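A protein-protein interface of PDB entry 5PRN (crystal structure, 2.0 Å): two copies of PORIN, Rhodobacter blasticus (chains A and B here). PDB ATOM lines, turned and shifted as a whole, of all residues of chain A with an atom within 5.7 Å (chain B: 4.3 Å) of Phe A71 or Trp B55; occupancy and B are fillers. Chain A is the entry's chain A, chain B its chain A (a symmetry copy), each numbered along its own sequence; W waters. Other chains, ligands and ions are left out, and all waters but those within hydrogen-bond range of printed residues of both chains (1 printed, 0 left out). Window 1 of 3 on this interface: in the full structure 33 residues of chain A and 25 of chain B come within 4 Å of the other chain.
Hydrophobic or aromatic side chains of chain A that line the printed part of chain B: Ala A49, Leu A51, Ala A68, Ala A69, Phe A71 and Val A82. Among the printed residues, 15 pairs touch across the chains.
O of Phe A71 sits at hydrogen-bond distance from N of Val A82, 2.8 Å away. O of Ala A68 sits at hydrogen-bond distance from ND2 of Asn A84, 3.2 Å away. The backbone carbonyl oxygen of Ala A69 is in hydrogen-bond range of the backbone NH of Asn A84, 3.0 Å away. O of Thr A73 lies within hydrogen-bond range of N of Val A80 (2.8 Å). The backbone NH of Ser B29 lies within hydrogen-bond range of the side-chain carboxylate of Asp B57 (2.9 Å). The side-chain amide nitrogen (NE2) of Gln B54 sits close to the guanidinium group (NE) of Arg B30.
No position is printed for both chains.
The backbone carbonyl oxygen (O) of Asn A67 lies within hydrogen-bond range of the side-chain hydroxyl (OG1) of Thr B64 (2.8 Å).
Among the printed residues, merely in contact across the chains: Phe A71 with Arg B30 (3.3 Å), Phe A71 with Ser B29 (3.4 Å), Gly A48 with Phe B287 (3.5 Å), Thr A73 with Phe B10 (3.5 Å), Ala A69 with Trp B55 (3.5 Å), Leu A51 with Thr B64 (3.6 Å), Ala A68 with Trp B55 (3.7 Å), Phe A71 with Phe B10 (3.7 Å), Ala A49 with Leu B31 (3.8 Å), Val A82 with Phe B10 (3.8 Å), Ala A69 with Leu B31 (3.8 Å), Phe A71 with Trp B55 (3.9 Å), Phe A71 with Leu B31 (3.95 Å) and Asn A67 with Gly B63 (3.97 Å).
Water W1 lies within hydrogen-bond range of the side-chain hydroxyl of Ser B29 (2.6 Å) and the side-chain amide oxygen of Asn A131 (3.0 Å).
Of the printed residues of chain B, Phe A71 touches Phe B10 (3.7 Å), Ser B29 (3.4 Å), Arg B30 (3.3 Å), Leu B31 (3.95 Å) and Trp B55 (3.9 Å). Trp B55 touches three residues of chain A. Of the printed residues of chain A, Thr B64 touches Leu A51 and Asn A67. Of the printed residues of chain B, Val A82 touches Phe B10 (3.8 Å). Ser A81 touches none of the printed residues of chain B. The nearest printed residue of chain B that does not touch Leu A51 is Leu B31 (4.01 Å).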
ATOM      1  N   GLY A  48       0.738 -35.496   4.180  1.00  0.00           N
ATOM      2  CA  GLY A  48       0.178 -34.436   4.996  1.00  0.00           C
ATOM      3  C   GLY A  48      -0.503 -33.374   4.140  1.00  0.00           C
ATOM      4  O   GLY A  48      -0.229 -33.233   2.942  1.00  0.00           O
ATOM      5  N   ALA A  49      -1.384 -32.669   4.803  1.00  0.00           N
ATOM      6  CA  ALA A  49      -2.112 -31.548   4.224  1.00  0.00           C
ATOM      7  C   ALA A  49      -2.172 -30.445   5.295  1.00  0.00           C
ATOM      8  O   ALA A  49      -2.280 -30.687   6.501  1.00  0.00           O
ATOM      9  CB  ALA A  49      -3.518 -31.974   3.805  1.00  0.00           C
ATOM     10  N   LYS A  50      -2.079 -29.192   4.789  1.00  0.00           N
ATOM     11  CA  LYS A  50      -2.214 -28.105   5.756  1.00  0.00           C
ATOM     12  C   LYS A  50      -3.023 -26.958   5.217  1.00  0.00           C
ATOM     13  O   LYS A  50      -3.078 -26.654   3.991  1.00  0.00           O
ATOM     14  CB  LYS A  50      -0.817 -27.782   6.201  1.00  0.00           C
ATOM     15  CG  LYS A  50      -0.267 -26.400   5.876  1.00  0.00           C
ATOM     16  CD  LYS A  50       1.268 -26.377   6.032  1.00  0.00           C
ATOM     17  CE  LYS A  50       1.824 -25.057   6.569  1.00  0.00           C
ATOM     18  NZ  LYS A  50       3.266 -25.116   6.871  1.00  0.00           N
ATOM     19  N   LEU A  51      -3.681 -26.295   6.163  1.00  0.00           N
ATOM     20  CA  LEU A  51      -4.501 -25.132   5.897  1.00  0.00           C
ATOM     21  C   LEU A  51      -4.142 -24.084   6.975  1.00  0.00           C
ATOM     22  O   LEU A  51      -3.939 -24.464   8.145  1.00  0.00           O
ATOM     23  CB  LEU A  51      -5.997 -25.465   5.960  1.00  0.00           C
ATOM     24  CG  LEU A  51      -6.978 -24.453   5.362  1.00  0.00           C
ATOM     25  CD1 LEU A  51      -6.874 -24.356   3.850  1.00  0.00           C
ATOM     26  CD2 LEU A  51      -8.421 -24.803   5.721  1.00  0.00           C
ATOM     27  N   ASN A  67      -6.839 -20.341   3.777  1.00  0.00           N
ATOM     28  CA  ASN A  67      -6.092 -20.061   2.548  1.00  0.00           C
ATOM     29  C   ASN A  67      -6.255 -21.254   1.599  1.00  0.00           C
ATOM     30  O   ASN A  67      -7.185 -22.093   1.763  1.00  0.00           O
ATOM     31  CB  ASN A  67      -4.650 -19.700   2.849  1.00  0.00           C
ATOM     32  CG  ASN A  67      -3.864 -20.799   3.512  1.00  0.00           C
ATOM     33  OD1 ASN A  67      -4.454 -21.794   4.005  1.00  0.00           O
ATOM     34  ND2 ASN A  67      -2.566 -20.641   3.584  1.00  0.00           N
ATOM     35  N   ALA A  68      -5.375 -21.376   0.609  1.00  0.00           N
ATOM     36  CA  ALA A  68      -5.397 -22.511  -0.299  1.00  0.00           C
ATOM     37  C   ALA A  68      -4.472 -23.575   0.297  1.00  0.00           C
ATOM     38  O   ALA A  68      -3.443 -23.269   0.922  1.00  0.00           O
ATOM     39  CB  ALA A  68      -4.888 -22.120  -1.702  1.00  0.00           C
ATOM     40  N   ALA A  69      -4.854 -24.820   0.049  1.00  0.00           N
ATOM     41  CA  ALA A  69      -4.178 -25.948   0.674  1.00  0.00           C
ATOM     42  C   ALA A  69      -2.773 -26.249   0.138  1.00  0.00           C
ATOM     43  O   ALA A  69      -2.365 -25.948  -0.983  1.00  0.00           O
ATOM     44  CB  ALA A  69      -5.025 -27.234   0.343  1.00  0.00           C
ATOM     45  N   GLN A  70      -2.018 -26.929   1.018  1.00  0.00           N
ATOM     46  CA  GLN A  70      -0.672 -27.372   0.669  1.00  0.00           C
ATOM     47  C   GLN A  70      -0.660 -28.895   0.953  1.00  0.00           C
ATOM     48  O   GLN A  70      -1.230 -29.271   2.010  1.00  0.00           O
ATOM     49  CB  GLN A  70       0.371 -26.651   1.499  1.00  0.00           C
ATOM     50  CG  GLN A  70       1.792 -27.243   1.268  1.00  0.00           C
ATOM     51  CD  GLN A  70       2.793 -26.649   2.223  1.00  0.00           C
ATOM     52  OE1 GLN A  70       3.290 -27.380   3.109  1.00  0.00           O
ATOM     53  NE2 GLN A  70       3.100 -25.359   2.155  1.00  0.00           N
ATOM     54  N   PHE A  71      -0.090 -29.719   0.113  1.00  0.00           N
ATOM     55  CA  PHE A  71      -0.039 -31.159   0.329  1.00  0.00           C
ATOM     56  C   PHE A  71       1.453 -31.586   0.308  1.00  0.00           C
ATOM     57  O   PHE A  71       2.227 -30.975  -0.405  1.00  0.00           O
ATOM     58  CB  PHE A  71      -0.781 -31.977  -0.728  1.00  0.00           C
ATOM     59  CG  PHE A  71      -2.198 -31.497  -0.933  1.00  0.00           C
ATOM     60  CD1 PHE A  71      -2.441 -30.450  -1.782  1.00  0.00           C
ATOM     61  CD2 PHE A  71      -3.259 -32.068  -0.246  1.00  0.00           C
ATOM     62  CE1 PHE A  71      -3.731 -29.904  -1.956  1.00  0.00           C
ATOM     63  CE2 PHE A  71      -4.556 -31.547  -0.434  1.00  0.00           C
ATOM     64  CZ  PHE A  71      -4.796 -30.495  -1.305  1.00  0.00           C
ATOM     65  N   TRP A  72       1.782 -32.650   1.032  1.00  0.00           N
ATOM     66  CA  TRP A  72       3.163 -33.125   0.972  1.00  0.00           C
ATOM     67  C   TRP A  72       3.230 -34.627   1.200  1.00  0.00           C
ATOM     68  O   TRP A  72       2.351 -35.241   1.788  1.00  0.00           O
ATOM     69  CB  TRP A  72       4.127 -32.400   1.887  1.00  0.00           C
ATOM     70  CG  TRP A  72       3.969 -32.751   3.330  1.00  0.00           C
ATOM     71  CD1 TRP A  72       4.570 -33.790   4.023  1.00  0.00           C
ATOM     72  CD2 TRP A  72       3.147 -32.064   4.275  1.00  0.00           C
ATOM     73  NE1 TRP A  72       4.148 -33.768   5.327  1.00  0.00           N
ATOM     74  CE2 TRP A  72       3.282 -32.715   5.501  1.00  0.00           C
ATOM     75  CE3 TRP A  72       2.305 -30.937   4.160  1.00  0.00           C
ATOM     76  CZ2 TRP A  72       2.609 -32.297   6.653  1.00  0.00           C
ATOM     77  CZ3 TRP A  72       1.640 -30.528   5.297  1.00  0.00           C
ATOM     78  CH2 TRP A  72       1.801 -31.210   6.516  1.00  0.00           C
ATOM     79  N   THR A  73       4.355 -35.173   0.712  1.00  0.00           N
ATOM     80  CA  THR A  73       4.723 -36.550   0.868  1.00  0.00           C
ATOM     81  C   THR A  73       6.213 -36.562   1.300  1.00  0.00           C
ATOM     82  O   THR A  73       7.020 -35.907   0.611  1.00  0.00           O
ATOM     83  CB  THR A  73       4.661 -37.350  -0.462  1.00  0.00           C
ATOM     84  OG1 THR A  73       3.351 -37.161  -1.045  1.00  0.00           O
ATOM     85  CG2 THR A  73       4.727 -38.838  -0.097  1.00  0.00           C
ATOM     86  N   VAL A  80       8.316 -33.850  -0.861  1.00  0.00           N
ATOM     87  CA  VAL A  80       7.793 -33.214  -2.080  1.00  0.00           C
ATOM     88  C   VAL A  80       6.433 -32.586  -1.688  1.00  0.00           C
ATOM     89  O   VAL A  80       5.615 -33.248  -1.068  1.00  0.00           O
ATOM     90  CB  VAL A  80       7.577 -34.229  -3.191  1.00  0.00           C
ATOM     91  CG1 VAL A  80       6.960 -33.618  -4.423  1.00  0.00           C
ATOM     92  CG2 VAL A  80       8.898 -34.942  -3.556  1.00  0.00           C
ATOM     93  N   SER A  81       6.258 -31.314  -1.989  1.00  0.00           N
ATOM     94  CA  SER A  81       5.050 -30.559  -1.661  1.00  0.00           C
ATOM     95  C   SER A  81       4.437 -30.020  -2.935  1.00  0.00           C
ATOM     96  O   SER A  81       5.064 -29.804  -3.964  1.00  0.00           O
ATOM     97  CB  SER A  81       5.237 -29.511  -0.570  1.00  0.00           C
ATOM     98  OG  SER A  81       6.336 -28.683  -0.928  1.00  0.00           O
ATOM     99  N   VAL A  82       3.101 -29.858  -2.870  1.00  0.00           N
ATOM    100  CA  VAL A  82       2.318 -29.423  -3.989  1.00  0.00           C
ATOM    101  C   VAL A  82       1.153 -28.515  -3.576  1.00  0.00           C
ATOM    102  O   VAL A  82       0.560 -28.712  -2.516  1.00  0.00           O
ATOM    103  CB  VAL A  82       1.706 -30.628  -4.764  1.00  0.00           C
ATOM    104  CG1 VAL A  82       2.749 -31.433  -5.544  1.00  0.00           C
ATOM    105  CG2 VAL A  82       0.852 -31.542  -3.890  1.00  0.00           C
ATOM    106  N   GLY A  83       0.880 -27.531  -4.437  1.00  0.00           N
ATOM    107  CA  GLY A  83      -0.213 -26.593  -4.254  1.00  0.00           C
ATOM    108  C   GLY A  83       0.304 -25.257  -3.787  1.00  0.00           C
ATOM    109  O   GLY A  83       1.056 -24.570  -4.492  1.00  0.00           O
ATOM    110  N   ASN A  84      -0.054 -24.876  -2.540  1.00  0.00           N
ATOM    111  CA  ASN A  84       0.438 -23.575  -1.990  1.00  0.00           C
ATOM    112  C   ASN A  84       1.715 -23.887  -1.235  1.00  0.00           C
ATOM    113  O   ASN A  84       1.690 -24.096  -0.012  1.00  0.00           O
ATOM    114  CB  ASN A  84      -0.615 -22.983  -1.054  1.00  0.00           C
ATOM    115  CG  ASN A  84      -0.317 -21.601  -0.477  1.00  0.00           C
ATOM    116  OD1 ASN A  84       0.682 -20.984  -0.826  1.00  0.00           O
ATOM    117  ND2 ASN A  84      -1.155 -21.077   0.405  1.00  0.00           N
ATOM    118  N   VAL A  85       2.857 -23.961  -1.899  1.00  0.00           N
ATOM    119  CA  VAL A  85       4.120 -24.349  -1.357  1.00  0.00           C
ATOM    120  C   VAL A  85       4.983 -23.229  -0.789  1.00  0.00           C
ATOM    121  O   VAL A  85       4.782 -22.049  -1.092  1.00  0.00           O
ATOM    122  CB  VAL A  85       4.964 -25.122  -2.427  1.00  0.00           C
ATOM    123  CG1 VAL A  85       4.099 -26.309  -2.994  1.00  0.00           C
ATOM    124  CG2 VAL A  85       5.325 -24.262  -3.649  1.00  0.00           C
ATOM    125  N   ASN A 131      -0.276 -22.688  -8.659  1.00  0.00           N
ATOM    126  CA  ASN A 131       0.072 -24.028  -8.151  1.00  0.00           C
ATOM    127  C   ASN A 131       1.560 -24.188  -8.176  1.00  0.00           C
ATOM    128  O   ASN A 131       2.164 -23.858  -9.225  1.00  0.00           O
ATOM    129  CB  ASN A 131      -0.604 -25.087  -9.035  1.00  0.00           C
ATOM    130  CG  ASN A 131      -0.454 -26.472  -8.429  1.00  0.00           C
ATOM    131  OD1 ASN A 131      -1.200 -26.754  -7.482  1.00  0.00           O
ATOM    132  ND2 ASN A 131       0.469 -27.267  -8.924  1.00  0.00           N
ATOM    133  N   GLY B   8      -6.963 -35.681   2.070  1.00  0.00           N
ATOM    134  CA  GLY B   8      -6.352 -34.815   1.040  1.00  0.00           C
ATOM    135  C   GLY B   8      -6.207 -35.755  -0.192  1.00  0.00           C
ATOM    136  O   GLY B   8      -6.131 -36.976  -0.046  1.00  0.00           O
ATOM    137  N   ARG B   9      -6.246 -35.169  -1.365  1.00  0.00           N
ATOM    138  CA  ARG B   9      -5.931 -35.897  -2.586  1.00  0.00           C
ATOM    139  C   ARG B   9      -5.228 -34.975  -3.573  1.00  0.00           C
ATOM    140  O   ARG B   9      -5.513 -33.780  -3.635  1.00  0.00           O
ATOM    141  CB  ARG B   9      -7.087 -36.632  -3.214  1.00  0.00           C
ATOM    142  CG  ARG B   9      -8.165 -35.731  -3.752  1.00  0.00           C
ATOM    143  CD  ARG B   9      -9.385 -36.510  -4.216  1.00  0.00           C
ATOM    144  NE  ARG B   9     -10.192 -35.706  -5.105  1.00  0.00           N
ATOM    145  CZ  ARG B   9     -11.456 -35.930  -5.423  1.00  0.00           C
ATOM    146  NH1 ARG B   9     -12.122 -36.979  -4.942  1.00  0.00           N
ATOM    147  NH2 ARG B   9     -12.140 -35.124  -6.242  1.00  0.00           N
ATOM    148  N   PHE B  10      -4.315 -35.586  -4.367  1.00  0.00           N
ATOM    149  CA  PHE B  10      -3.665 -34.772  -5.410  1.00  0.00           C
ATOM    150  C   PHE B  10      -3.205 -35.684  -6.543  1.00  0.00           C
ATOM    151  O   PHE B  10      -2.991 -36.895  -6.306  1.00  0.00           O
ATOM    152  CB  PHE B  10      -2.525 -33.912  -4.822  1.00  0.00           C
ATOM    153  CG  PHE B  10      -1.345 -34.649  -4.277  1.00  0.00           C
ATOM    154  CD1 PHE B  10      -0.349 -35.115  -5.115  1.00  0.00           C
ATOM    155  CD2 PHE B  10      -1.203 -34.898  -2.930  1.00  0.00           C
ATOM    156  CE1 PHE B  10       0.716 -35.848  -4.630  1.00  0.00           C
ATOM    157  CE2 PHE B  10      -0.104 -35.577  -2.418  1.00  0.00           C
ATOM    158  CZ  PHE B  10       0.872 -36.058  -3.271  1.00  0.00           C
ATOM    159  N   SER B  29      -6.361 -31.141  -7.103  1.00  0.00           N
ATOM    160  CA  SER B  29      -6.174 -31.491  -5.694  1.00  0.00           C
ATOM    161  C   SER B  29      -7.335 -30.976  -4.855  1.00  0.00           C
ATOM    162  O   SER B  29      -8.143 -30.133  -5.335  1.00  0.00           O
ATOM    163  CB  SER B  29      -4.823 -31.004  -5.171  1.00  0.00           C
ATOM    164  OG  SER B  29      -4.705 -29.588  -5.225  1.00  0.00           O
ATOM    165  N   ARG B  30      -7.554 -31.666  -3.742  1.00  0.00           N
ATOM    166  CA  ARG B  30      -8.688 -31.318  -2.891  1.00  0.00           C
ATOM    167  C   ARG B  30      -8.283 -31.499  -1.428  1.00  0.00           C
ATOM    168  O   ARG B  30      -7.650 -32.502  -1.116  1.00  0.00           O
ATOM    169  CB  ARG B  30      -9.884 -32.250  -3.202  1.00  0.00           C
ATOM    170  CG  ARG B  30     -11.034 -32.066  -2.199  1.00  0.00           C
ATOM    171  CD  ARG B  30     -12.174 -32.974  -2.544  1.00  0.00           C
ATOM    172  NE  ARG B  30     -12.856 -32.535  -3.796  1.00  0.00           N
ATOM    173  CZ  ARG B  30     -13.911 -33.194  -4.269  1.00  0.00           C
ATOM    174  NH1 ARG B  30     -14.401 -34.278  -3.668  1.00  0.00           N
ATOM    175  NH2 ARG B  30     -14.479 -32.777  -5.397  1.00  0.00           N
ATOM    176  N   LEU B  31      -8.675 -30.597  -0.551  1.00  0.00           N
ATOM    177  CA  LEU B  31      -8.549 -30.802   0.867  1.00  0.00           C
ATOM    178  C   LEU B  31      -9.966 -30.739   1.484  1.00  0.00           C
ATOM    179  O   LEU B  31     -10.697 -29.754   1.166  1.00  0.00           O
ATOM    180  CB  LEU B  31      -7.647 -29.782   1.529  1.00  0.00           C
ATOM    181  CG  LEU B  31      -7.732 -29.744   3.107  1.00  0.00           C
ATOM    182  CD1 LEU B  31      -7.160 -31.028   3.640  1.00  0.00           C
ATOM    183  CD2 LEU B  31      -6.931 -28.534   3.548  1.00  0.00           C
ATOM    184  N   GLN B  54     -14.036 -27.284   2.608  1.00  0.00           N
ATOM    185  CA  GLN B  54     -13.414 -27.990   1.488  1.00  0.00           C
ATOM    186  C   GLN B  54     -12.791 -26.989   0.526  1.00  0.00           C
ATOM    187  O   GLN B  54     -13.460 -26.005   0.161  1.00  0.00           O
ATOM    188  CB  GLN B  54     -14.479 -28.804   0.725  1.00  0.00           C
ATOM    189  CG  GLN B  54     -13.850 -29.641  -0.419  1.00  0.00           C
ATOM    190  CD  GLN B  54     -14.861 -30.544  -1.047  1.00  0.00           C
ATOM    191  OE1 GLN B  54     -15.532 -31.304  -0.310  1.00  0.00           O
ATOM    192  NE2 GLN B  54     -15.019 -30.491  -2.390  1.00  0.00           N
ATOM    193  N   TRP B  55     -11.596 -27.273   0.054  1.00  0.00           N
ATOM    194  CA  TRP B  55     -10.906 -26.485  -0.948  1.00  0.00           C
ATOM    195  C   TRP B  55     -10.598 -27.403  -2.140  1.00  0.00           C
ATOM    196  O   TRP B  55     -10.182 -28.575  -1.998  1.00  0.00           O
ATOM    197  CB  TRP B  55      -9.583 -25.886  -0.363  1.00  0.00           C
ATOM    198  CG  TRP B  55      -8.775 -25.210  -1.472  1.00  0.00           C
ATOM    199  CD1 TRP B  55      -8.900 -23.910  -1.867  1.00  0.00           C
ATOM    200  CD2 TRP B  55      -7.741 -25.780  -2.287  1.00  0.00           C
ATOM    201  NE1 TRP B  55      -8.027 -23.615  -2.876  1.00  0.00           N
ATOM    202  CE2 TRP B  55      -7.284 -24.760  -3.157  1.00  0.00           C
ATOM    203  CE3 TRP B  55      -7.185 -27.049  -2.425  1.00  0.00           C
ATOM    204  CZ2 TRP B  55      -6.315 -24.980  -4.129  1.00  0.00           C
ATOM    205  CZ3 TRP B  55      -6.223 -27.294  -3.396  1.00  0.00           C
ATOM    206  CH2 TRP B  55      -5.786 -26.231  -4.253  1.00  0.00           C
ATOM    207  N   ASP B  56     -10.783 -26.901  -3.339  1.00  0.00           N
ATOM    208  CA  ASP B  56     -10.414 -27.551  -4.610  1.00  0.00           C
ATOM    209  C   ASP B  56      -9.559 -26.631  -5.458  1.00  0.00           C
ATOM    210  O   ASP B  56      -9.728 -25.416  -5.408  1.00  0.00           O
ATOM    211  CB  ASP B  56     -11.661 -27.961  -5.422  1.00  0.00           C
ATOM    212  CG  ASP B  56     -12.411 -29.142  -4.786  1.00  0.00           C
ATOM    213  OD1 ASP B  56     -13.343 -28.919  -3.965  1.00  0.00           O
ATOM    214  OD2 ASP B  56     -12.171 -30.281  -5.142  1.00  0.00           O
ATOM    215  N   ASP B  57      -8.652 -27.190  -6.281  1.00  0.00           N
ATOM    216  CA  ASP B  57      -7.822 -26.314  -7.130  1.00  0.00           C
ATOM    217  C   ASP B  57      -8.759 -25.504  -8.032  1.00  0.00           C
ATOM    218  O   ASP B  57      -9.793 -26.047  -8.412  1.00  0.00           O
ATOM    219  CB  ASP B  57      -6.842 -27.141  -8.010  1.00  0.00           C
ATOM    220  CG  ASP B  57      -7.571 -28.100  -8.883  1.00  0.00           C
ATOM    221  OD1 ASP B  57      -8.046 -29.205  -8.475  1.00  0.00           O
ATOM    222  OD2 ASP B  57      -7.779 -27.806 -10.100  1.00  0.00           O
ATOM    223  N   ASP B  59     -10.513 -22.968  -7.025  1.00  0.00           N
ATOM    224  CA  ASP B  59     -11.583 -22.287  -6.271  1.00  0.00           C
ATOM    225  C   ASP B  59     -11.315 -20.774  -6.250  1.00  0.00           C
ATOM    226  O   ASP B  59     -10.206 -20.306  -6.130  1.00  0.00           O
ATOM    227  CB  ASP B  59     -11.679 -22.709  -4.773  1.00  0.00           C
ATOM    228  CG  ASP B  59     -12.506 -23.957  -4.585  1.00  0.00           C
ATOM    229  OD1 ASP B  59     -13.080 -24.469  -5.523  1.00  0.00           O
ATOM    230  OD2 ASP B  59     -12.560 -24.479  -3.429  1.00  0.00           O
ATOM    231  N   GLY B  63      -9.196 -19.360  -1.440  1.00  0.00           N
ATOM    232  CA  GLY B  63      -9.545 -19.423   0.004  1.00  0.00           C
ATOM    233  C   GLY B  63     -10.537 -20.569   0.274  1.00  0.00           C
ATOM    234  O   GLY B  63     -11.037 -21.246  -0.640  1.00  0.00           O
ATOM    235  N   THR B  64     -10.735 -20.818   1.571  1.00  0.00           N
ATOM    236  CA  THR B  64     -11.573 -21.929   1.989  1.00  0.00           C
ATOM    237  C   THR B  64     -12.499 -21.372   3.083  1.00  0.00           C
ATOM    238  O   THR B  64     -12.014 -20.658   3.988  1.00  0.00           O
ATOM    239  CB  THR B  64     -10.676 -23.021   2.637  1.00  0.00           C
ATOM    240  OG1 THR B  64      -9.646 -23.359   1.708  1.00  0.00           O
ATOM    241  CG2 THR B  64     -11.401 -24.329   3.009  1.00  0.00           C
ATOM    242  N   LYS B 120     -19.992 -26.612  -0.183  1.00  0.00           N
ATOM    243  CA  LYS B 120     -19.418 -25.321  -0.049  1.00  0.00           C
ATOM    244  C   LYS B 120     -20.465 -24.211  -0.049  1.00  0.00           C
ATOM    245  O   LYS B 120     -21.659 -24.506  -0.294  1.00  0.00           O
ATOM    246  CB  LYS B 120     -18.532 -25.066  -1.325  1.00  0.00           C
ATOM    247  CG  LYS B 120     -17.272 -25.947  -1.357  1.00  0.00           C
ATOM    248  CD  LYS B 120     -16.403 -25.647  -2.593  1.00  0.00           C
ATOM    249  CE  LYS B 120     -15.325 -26.704  -2.701  1.00  0.00           C
ATOM    250  NZ  LYS B 120     -14.406 -26.463  -3.821  1.00  0.00           N
ATOM    251  N   PHE B 287      -5.324 -39.688   0.740  1.00  0.00           N
ATOM    252  CA  PHE B 287      -4.940 -40.074   2.079  1.00  0.00           C
ATOM    253  C   PHE B 287      -5.927 -39.506   3.093  1.00  0.00           C
ATOM    254  O   PHE B 287      -6.322 -38.338   3.048  1.00  0.00           O
ATOM    255  CB  PHE B 287      -3.467 -39.734   2.362  1.00  0.00           C
ATOM    256  CG  PHE B 287      -3.139 -38.262   2.143  1.00  0.00           C
ATOM    257  CD1 PHE B 287      -2.820 -37.771   0.914  1.00  0.00           C
ATOM    258  CD2 PHE B 287      -3.202 -37.407   3.244  1.00  0.00           C
ATOM    259  CE1 PHE B 287      -2.493 -36.423   0.735  1.00  0.00           C
ATOM    260  CE2 PHE B 287      -2.862 -36.069   3.076  1.00  0.00           C
ATOM    261  CZ  PHE B 287      -2.532 -35.585   1.822  1.00  0.00           C
HETATM  262  O   HOH W   1      -3.563 -28.538  -7.357  1.00  0.00           O
